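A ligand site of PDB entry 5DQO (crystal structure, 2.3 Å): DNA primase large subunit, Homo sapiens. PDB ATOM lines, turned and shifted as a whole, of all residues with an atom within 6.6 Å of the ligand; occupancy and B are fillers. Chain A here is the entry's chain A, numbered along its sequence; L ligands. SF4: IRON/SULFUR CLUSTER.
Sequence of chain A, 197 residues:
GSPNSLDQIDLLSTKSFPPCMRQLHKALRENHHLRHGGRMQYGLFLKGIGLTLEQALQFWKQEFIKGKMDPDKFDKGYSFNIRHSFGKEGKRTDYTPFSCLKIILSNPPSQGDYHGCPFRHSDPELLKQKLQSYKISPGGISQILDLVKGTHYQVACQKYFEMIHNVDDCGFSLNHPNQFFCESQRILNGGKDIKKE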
ATOM      1  N   PRO A  18       3.158  24.745  -9.631  1.00  0.00           N
ATOM      2  CA  PRO A  18       3.541  24.855 -11.029  1.00  0.00           C
ATOM      3  C   PRO A  18       2.761  26.003 -11.621  1.00  0.00           C
ATOM      4  O   PRO A  18       2.035  26.688 -10.899  1.00  0.00           O
ATOM      5  CB  PRO A  18       3.056  23.525 -11.619  1.00  0.00           C
ATOM      6  CG  PRO A  18       1.895  23.141 -10.760  1.00  0.00           C
ATOM      7  CD  PRO A  18       2.236  23.620  -9.376  1.00  0.00           C
ATOM      8  N   PRO A  19       2.905  26.215 -12.920  1.00  0.00           N
ATOM      9  CA  PRO A  19       2.165  27.317 -13.568  1.00  0.00           C
ATOM     10  C   PRO A  19       0.660  27.129 -13.762  1.00  0.00           C
ATOM     11  O   PRO A  19      -0.059  28.088 -14.025  1.00  0.00           O
ATOM     12  CB  PRO A  19       2.861  27.436 -14.931  1.00  0.00           C
ATOM     13  CG  PRO A  19       4.236  26.931 -14.694  1.00  0.00           C
ATOM     14  CD  PRO A  19       4.108  25.833 -13.675  1.00  0.00           C
ATOM     15  N   CYS A  20       0.233  25.851 -13.656  1.00  0.00           N
ATOM     16  CA  CYS A  20      -1.103  25.503 -13.822  1.00  0.00           C
ATOM     17  C   CYS A  20      -1.813  25.518 -12.530  1.00  0.00           C
ATOM     18  O   CYS A  20      -3.036  25.600 -12.510  1.00  0.00           O
ATOM     19  CB  CYS A  20      -1.251  24.099 -14.397  1.00  0.00           C
ATOM     20  SG  CYS A  20      -0.252  22.896 -13.542  1.00  0.00           S
ATOM     21  N   MET A  21      -1.096  25.459 -11.434  1.00  0.00           N
ATOM     22  CA  MET A  21      -1.702  25.434 -10.137  1.00  0.00           C
ATOM     23  C   MET A  21      -1.639  26.749  -9.509  1.00  0.00           C
ATOM     24  O   MET A  21      -2.507  27.084  -8.802  1.00  0.00           O
ATOM     25  CB  MET A  21      -1.082  24.388  -9.276  1.00  0.00           C
ATOM     26  CG  MET A  21      -1.107  23.047  -9.915  1.00  0.00           C
ATOM     27  SD  MET A  21      -2.735  22.470 -10.219  1.00  0.00           S
ATOM     28  CE  MET A  21      -2.453  20.831 -10.798  1.00  0.00           C
ATOM     29  N   GLN A  41      -8.794  20.035 -11.311  1.00  0.00           N
ATOM     30  CA  GLN A  41      -7.384  20.100 -11.539  1.00  0.00           C
ATOM     31  C   GLN A  41      -6.783  20.569 -10.253  1.00  0.00           C
ATOM     32  O   GLN A  41      -5.859  20.008  -9.786  1.00  0.00           O
ATOM     33  CB  GLN A  41      -7.034  21.025 -12.682  1.00  0.00           C
ATOM     34  CG  GLN A  41      -5.551  21.170 -12.955  1.00  0.00           C
ATOM     35  CD  GLN A  41      -5.252  22.028 -14.142  1.00  0.00           C
ATOM     36  OE1 GLN A  41      -5.971  22.047 -15.067  1.00  0.00           O
ATOM     37  NE2 GLN A  41      -4.178  22.728 -14.094  1.00  0.00           N
ATOM     38  N   SER A  99      -1.798  14.264 -14.370  1.00  0.00           N
ATOM     39  CA  SER A  99      -0.425  14.241 -14.830  1.00  0.00           C
ATOM     40  C   SER A  99      -0.204  15.398 -15.756  1.00  0.00           C
ATOM     41  O   SER A  99      -1.123  16.039 -16.080  1.00  0.00           O
ATOM     42  CB  SER A  99      -0.096  12.917 -15.486  1.00  0.00           C
ATOM     43  OG  SER A  99      -0.869  12.634 -16.590  1.00  0.00           O
ATOM     44  N   CYS A 100       1.012  15.660 -16.178  1.00  0.00           N
ATOM     45  CA  CYS A 100       1.285  16.789 -17.053  1.00  0.00           C
ATOM     46  C   CYS A 100       0.626  16.576 -18.383  1.00  0.00           C
ATOM     47  O   CYS A 100       0.024  17.463 -18.899  1.00  0.00           O
ATOM     48  CB  CYS A 100       2.780  17.142 -17.094  1.00  0.00           C
ATOM     49  SG  CYS A 100       3.429  17.908 -15.616  1.00  0.00           S
ATOM     50  N   LEU A 101       0.743  15.377 -18.880  1.00  0.00           N
ATOM     51  CA  LEU A 101       0.124  14.891 -20.099  1.00  0.00           C
ATOM     52  C   LEU A 101      -1.378  14.832 -20.116  1.00  0.00           C
ATOM     53  O   LEU A 101      -2.017  15.132 -21.156  1.00  0.00           O
ATOM     54  CB  LEU A 101       0.664  13.487 -20.455  1.00  0.00           C
ATOM     55  CG  LEU A 101       2.026  13.395 -21.162  1.00  0.00           C
ATOM     56  CD1 LEU A 101       2.144  12.059 -21.901  1.00  0.00           C
ATOM     57  CD2 LEU A 101       2.249  14.527 -22.194  1.00  0.00           C
ATOM     58  N   ILE A 103      -3.381  16.845 -18.328  1.00  0.00           N
ATOM     59  CA  ILE A 103      -3.717  18.232 -18.377  1.00  0.00           C
ATOM     60  C   ILE A 103      -3.451  18.828 -19.729  1.00  0.00           C
ATOM     61  O   ILE A 103      -4.250  19.532 -20.238  1.00  0.00           O
ATOM     62  CB  ILE A 103      -2.922  19.009 -17.303  1.00  0.00           C
ATOM     63  CG1 ILE A 103      -3.441  18.710 -15.924  1.00  0.00           C
ATOM     64  CG2 ILE A 103      -3.105  20.491 -17.433  1.00  0.00           C
ATOM     65  CD1 ILE A 103      -2.701  19.395 -14.842  1.00  0.00           C
ATOM     66  N   ILE A 104      -2.291  18.567 -20.289  1.00  0.00           N
ATOM     67  CA  ILE A 104      -1.907  19.092 -21.562  1.00  0.00           C
ATOM     68  C   ILE A 104      -2.687  18.496 -22.717  1.00  0.00           C
ATOM     69  O   ILE A 104      -3.019  19.200 -23.591  1.00  0.00           O
ATOM     70  CB  ILE A 104      -0.395  18.916 -21.786  1.00  0.00           C
ATOM     71  CG1 ILE A 104       0.386  19.854 -20.918  1.00  0.00           C
ATOM     72  CG2 ILE A 104       0.022  19.156 -23.221  1.00  0.00           C
ATOM     73  CD1 ILE A 104       1.862  19.781 -21.128  1.00  0.00           C
ATOM     74  N   GLY A 116      -5.843  23.776 -17.147  1.00  0.00           N
ATOM     75  CA  GLY A 116      -4.884  23.291 -18.137  1.00  0.00           C
ATOM     76  C   GLY A 116      -3.424  23.725 -17.953  1.00  0.00           C
ATOM     77  O   GLY A 116      -3.126  24.315 -16.974  1.00  0.00           O
ATOM     78  N   CYS A 117      -2.508  23.422 -18.871  1.00  0.00           N
ATOM     79  CA  CYS A 117      -1.128  23.884 -18.783  1.00  0.00           C
ATOM     80  C   CYS A 117      -1.074  25.241 -19.424  1.00  0.00           C
ATOM     81  O   CYS A 117      -1.584  25.442 -20.479  1.00  0.00           O
ATOM     82  CB  CYS A 117      -0.085  22.987 -19.483  1.00  0.00           C
ATOM     83  SG  CYS A 117       1.620  23.614 -19.581  1.00  0.00           S
ATOM     84  N   PRO A 118      -0.416  26.185 -18.773  1.00  0.00           N
ATOM     85  CA  PRO A 118      -0.277  27.543 -19.315  1.00  0.00           C
ATOM     86  C   PRO A 118       0.637  27.520 -20.535  1.00  0.00           C
ATOM     87  O   PRO A 118       0.257  27.996 -21.608  1.00  0.00           O
ATOM     88  CB  PRO A 118       0.393  28.296 -18.172  1.00  0.00           C
ATOM     89  CG  PRO A 118      -0.042  27.581 -16.941  1.00  0.00           C
ATOM     90  CD  PRO A 118      -0.140  26.129 -17.334  1.00  0.00           C
ATOM     91  N   PHE A 119       1.828  26.960 -20.377  1.00  0.00           N
ATOM     92  CA  PHE A 119       2.792  26.840 -21.451  1.00  0.00           C
ATOM     93  C   PHE A 119       2.201  26.217 -22.659  1.00  0.00           C
ATOM     94  O   PHE A 119       2.688  26.409 -23.711  1.00  0.00           O
ATOM     95  CB  PHE A 119       3.976  25.966 -21.070  1.00  0.00           C
ATOM     96  CG  PHE A 119       4.678  26.399 -19.860  1.00  0.00           C
ATOM     97  CD1 PHE A 119       5.498  27.480 -19.892  1.00  0.00           C
ATOM     98  CD2 PHE A 119       4.523  25.730 -18.690  1.00  0.00           C
ATOM     99  CE1 PHE A 119       6.141  27.903 -18.750  1.00  0.00           C
ATOM    100  CE2 PHE A 119       5.172  26.141 -17.567  1.00  0.00           C
ATOM    101  CZ  PHE A 119       5.978  27.221 -17.596  1.00  0.00           C
ATOM    102  N   ARG A 120       1.138  25.467 -22.503  1.00  0.00           N
ATOM    103  CA  ARG A 120       0.532  24.834 -23.616  1.00  0.00           C
ATOM    104  C   ARG A 120      -0.713  25.575 -24.062  1.00  0.00           C
ATOM    105  O   ARG A 120      -0.926  25.750 -25.214  1.00  0.00           O
ATOM    106  CB  ARG A 120       0.278  23.386 -23.308  1.00  0.00           C
ATOM    107  CG  ARG A 120      -0.901  22.762 -23.984  1.00  0.00           C
ATOM    108  CD  ARG A 120      -0.666  22.763 -25.442  1.00  0.00           C
ATOM    109  NE  ARG A 120      -1.710  22.048 -26.088  1.00  0.00           N
ATOM    110  CZ  ARG A 120      -2.570  22.609 -26.884  1.00  0.00           C
ATOM    111  NH1 ARG A 120      -2.492  23.877 -27.136  1.00  0.00           N
ATOM    112  NH2 ARG A 120      -3.507  21.893 -27.421  1.00  0.00           N
ATOM    113  N   TYR A 153       6.475  21.917 -23.783  1.00  0.00           N
ATOM    114  CA  TYR A 153       5.879  22.604 -22.676  1.00  0.00           C
ATOM    115  C   TYR A 153       6.350  22.156 -21.331  1.00  0.00           C
ATOM    116  O   TYR A 153       6.541  22.948 -20.476  1.00  0.00           O
ATOM    117  CB  TYR A 153       4.353  22.531 -22.725  1.00  0.00           C
ATOM    118  CG  TYR A 153       3.793  22.659 -24.092  1.00  0.00           C
ATOM    119  CD1 TYR A 153       3.914  23.817 -24.802  1.00  0.00           C
ATOM    120  CD2 TYR A 153       3.166  21.628 -24.682  1.00  0.00           C
ATOM    121  CE1 TYR A 153       3.421  23.924 -26.062  1.00  0.00           C
ATOM    122  CE2 TYR A 153       2.673  21.743 -25.930  1.00  0.00           C
ATOM    123  CZ  TYR A 153       2.803  22.906 -26.618  1.00  0.00           C
ATOM    124  OH  TYR A 153       2.296  23.011 -27.875  1.00  0.00           O
ATOM    125  N   GLN A 154       6.563  20.865 -21.169  1.00  0.00           N
ATOM    126  CA  GLN A 154       7.050  20.355 -19.912  1.00  0.00           C
ATOM    127  C   GLN A 154       8.453  20.850 -19.681  1.00  0.00           C
ATOM    128  O   GLN A 154       8.816  21.131 -18.593  1.00  0.00           O
ATOM    129  CB  GLN A 154       6.986  18.816 -19.848  1.00  0.00           C
ATOM    130  CG  GLN A 154       5.663  18.228 -19.435  1.00  0.00           C
ATOM    131  CD  GLN A 154       5.357  16.919 -20.113  1.00  0.00           C
ATOM    132  OE1 GLN A 154       5.072  16.895 -21.245  1.00  0.00           O
ATOM    133  NE2 GLN A 154       5.403  15.843 -19.386  1.00  0.00           N
ATOM    134  N   VAL A 155       9.242  20.993 -20.708  1.00  0.00           N
ATOM    135  CA  VAL A 155      10.580  21.465 -20.440  1.00  0.00           C
ATOM    136  C   VAL A 155      10.486  22.999 -20.296  1.00  0.00           C
ATOM    137  O   VAL A 155      11.255  23.705 -19.573  1.00  0.00           O
ATOM    138  CB  VAL A 155      11.561  21.030 -21.555  1.00  0.00           C
ATOM    139  CG1 VAL A 155      13.013  21.011 -21.047  1.00  0.00           C
ATOM    140  CG2 VAL A 155      11.150  19.696 -22.068  1.00  0.00           C
ATOM    141  N   ALA A 156       9.513  23.558 -20.978  1.00  0.00           N
ATOM    142  CA  ALA A 156       9.249  24.967 -20.740  1.00  0.00           C
ATOM    143  C   ALA A 156       9.027  25.172 -19.259  1.00  0.00           C
ATOM    144  O   ALA A 156       9.499  26.139 -18.700  1.00  0.00           O
ATOM    145  CB  ALA A 156       8.116  25.513 -21.604  1.00  0.00           C
ATOM    146  N   CYS A 157       8.383  24.231 -18.613  1.00  0.00           N
ATOM    147  CA  CYS A 157       8.129  24.277 -17.154  1.00  0.00           C
ATOM    148  C   CYS A 157       9.366  23.950 -16.272  1.00  0.00           C
ATOM    149  O   CYS A 157       9.468  24.403 -15.189  1.00  0.00           O
ATOM    150  CB  CYS A 157       6.904  23.427 -16.835  1.00  0.00           C
ATOM    151  SG  CYS A 157       6.775  22.588 -15.216  1.00  0.00           S
ATOM    152  N   GLN A 158      10.320  23.219 -16.773  1.00  0.00           N
ATOM    153  CA  GLN A 158      11.511  22.988 -16.004  1.00  0.00           C
ATOM    154  C   GLN A 158      12.285  24.275 -15.964  1.00  0.00           C
ATOM    155  O   GLN A 158      12.876  24.568 -14.988  1.00  0.00           O
ATOM    156  CB  GLN A 158      12.345  21.848 -16.556  1.00  0.00           C
ATOM    157  CG  GLN A 158      11.692  20.513 -16.419  1.00  0.00           C
ATOM    158  CD  GLN A 158      12.269  19.485 -17.318  1.00  0.00           C
ATOM    159  OE1 GLN A 158      13.410  19.523 -17.649  1.00  0.00           O
ATOM    160  NE2 GLN A 158      11.483  18.543 -17.690  1.00  0.00           N
ATOM    161  N   LEU A 174      10.320  16.164 -15.600  1.00  0.00           N
ATOM    162  CA  LEU A 174       9.036  16.478 -15.071  1.00  0.00           C
ATOM    163  C   LEU A 174       7.891  15.730 -15.738  1.00  0.00           C
ATOM    164  O   LEU A 174       7.854  15.597 -16.913  1.00  0.00           O
ATOM    165  CB  LEU A 174       8.818  17.962 -15.190  1.00  0.00           C
ATOM    166  CG  LEU A 174       7.459  18.494 -14.807  1.00  0.00           C
ATOM    167  CD1 LEU A 174       7.451  19.136 -13.451  1.00  0.00           C
ATOM    168  CD2 LEU A 174       6.932  19.444 -15.841  1.00  0.00           C
ATOM    169  N   ASN A 175       6.960  15.260 -14.936  1.00  0.00           N
ATOM    170  CA  ASN A 175       5.823  14.502 -15.394  1.00  0.00           C
ATOM    171  C   ASN A 175       4.571  14.895 -14.678  1.00  0.00           C
ATOM    172  O   ASN A 175       3.540  14.806 -15.223  1.00  0.00           O
ATOM    173  CB  ASN A 175       6.072  13.003 -15.477  1.00  0.00           C
ATOM    174  CG  ASN A 175       6.287  12.366 -14.152  1.00  0.00           C
ATOM    175  OD1 ASN A 175       5.400  12.240 -13.369  1.00  0.00           O
ATOM    176  ND2 ASN A 175       7.466  11.941 -13.926  1.00  0.00           N
ATOM    177  N   HIS A 176       4.694  15.327 -13.457  1.00  0.00           N
ATOM    178  CA  HIS A 176       3.543  15.603 -12.654  1.00  0.00           C
ATOM    179  C   HIS A 176       3.637  16.889 -11.918  1.00  0.00           C
ATOM    180  O   HIS A 176       4.587  17.123 -11.291  1.00  0.00           O
ATOM    181  CB  HIS A 176       3.348  14.474 -11.626  1.00  0.00           C
ATOM    182  CG  HIS A 176       1.925  14.143 -11.298  1.00  0.00           C
ATOM    183  ND1 HIS A 176       1.079  15.020 -10.693  1.00  0.00           N
ATOM    184  CD2 HIS A 176       1.217  13.017 -11.478  1.00  0.00           C
ATOM    185  CE1 HIS A 176      -0.100  14.456 -10.526  1.00  0.00           C
ATOM    186  NE2 HIS A 176      -0.038  13.244 -11.010  1.00  0.00           N
ATOM    187  N   PRO A 177       2.631  17.701 -11.966  1.00  0.00           N
ATOM    188  CA  PRO A 177       2.643  18.947 -11.231  1.00  0.00           C
ATOM    189  C   PRO A 177       3.002  18.722  -9.770  1.00  0.00           C
ATOM    190  O   PRO A 177       3.660  19.515  -9.174  1.00  0.00           O
ATOM    191  CB  PRO A 177       1.218  19.444 -11.362  1.00  0.00           C
ATOM    192  CG  PRO A 177       0.782  18.916 -12.634  1.00  0.00           C
ATOM    193  CD  PRO A 177       1.470  17.613 -12.837  1.00  0.00           C
ATOM    194  N   ASN A 178       2.508  17.610  -9.245  1.00  0.00           N
ATOM    195  CA  ASN A 178       2.742  17.250  -7.853  1.00  0.00           C
ATOM    196  C   ASN A 178       4.186  16.847  -7.615  1.00  0.00           C
ATOM    197  O   ASN A 178       4.664  16.885  -6.479  1.00  0.00           O
ATOM    198  CB  ASN A 178       1.800  16.116  -7.432  1.00  0.00           C
ATOM    199  CG  ASN A 178       0.421  16.609  -7.063  1.00  0.00           C
ATOM    200  OD1 ASN A 178      -0.540  16.410  -7.795  1.00  0.00           O
ATOM    201  ND2 ASN A 178       0.322  17.254  -5.905  1.00  0.00           N
ATOM    202  N   PHE A 180       6.566  18.356  -9.189  1.00  0.00           N
ATOM    203  CA  PHE A 180       7.170  19.659  -9.237  1.00  0.00           C
ATOM    204  C   PHE A 180       7.063  20.177  -7.853  1.00  0.00           C
ATOM    205  O   PHE A 180       7.960  20.741  -7.395  1.00  0.00           O
ATOM    206  CB  PHE A 180       6.407  20.551 -10.204  1.00  0.00           C
ATOM    207  CG  PHE A 180       6.844  21.989 -10.279  1.00  0.00           C
ATOM    208  CD1 PHE A 180       6.749  22.818  -9.230  1.00  0.00           C
ATOM    209  CD2 PHE A 180       7.257  22.522 -11.481  1.00  0.00           C
ATOM    210  CE1 PHE A 180       7.103  24.105  -9.338  1.00  0.00           C
ATOM    211  CE2 PHE A 180       7.638  23.828 -11.587  1.00  0.00           C
ATOM    212  CZ  PHE A 180       7.542  24.620 -10.519  1.00  0.00           C
HETATM  213 FE1  SF4 L   1       1.703  22.434 -14.622  1.00  0.00          FE
HETATM  214 FE2  SF4 L   1       3.168  20.205 -16.032  1.00  0.00          FE
HETATM  215 FE3  SF4 L   1       4.537  22.859 -15.586  1.00  0.00          FE
HETATM  216 FE4  SF4 L   1       2.279  22.643 -17.574  1.00  0.00          FE
HETATM  217  S1  SF4 L   1       4.143  21.639 -17.291  1.00  0.00           S
HETATM  218  S2  SF4 L   1       2.678  23.868 -15.881  1.00  0.00           S
HETATM  219  S3  SF4 L   1       1.309  21.214 -16.327  1.00  0.00           S
HETATM  220  S4  SF4 L   1       3.567  21.430 -14.339  1.00  0.00           S
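The backbone nitrogen of Pro 19 lies close to a sulfur (S2) of the ligand, at 3.8 Å. Pro 18 touches the ligand (CB to FE1, 3.5 Å). Pro 118 touches the ligand. Phe 119 touches the ligand (CE2 to S2, 3.8 Å). Leu 174 touches the ligand (CD2 to S1, 3.8 Å).
The side-chain amide nitrogen of Gln 41 lies close to the backbone carbonyl oxygen of Cys 20 (3.5 Å). SG of Cys 117 sits close to N of Phe 119 (3.4 Å). N of Arg 120 lies close to SG of Cys 117. The side-chain sulfur (SG) of Cys 100 lies close to the backbone NH (N) of His 176, at 3.6 Å. The backbone carbonyl oxygen (O) of Asn 175 is in hydrogen-bond range of the backbone NH (N) of Cys 100 (2.8 Å). The backbone carbonyl oxygen (O) of Leu 174 is in hydrogen-bond range of the side-chain amide nitrogen (NE2) of Gln 154 (3.5 Å). NE2 of Gln 158 sits close to N of Leu 174, 3.4 Å away.
SG of Cys 20 binds FE1 of the ligand, 2.3 Å away. SG of Cys 157 binds FE3 of the ligand, at 2.3 Å. SG of Cys 117 binds FE4 of the ligand. An iron atom (FE2) of the ligand is bound by the side-chain sulfur (SG) of Cys 100.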
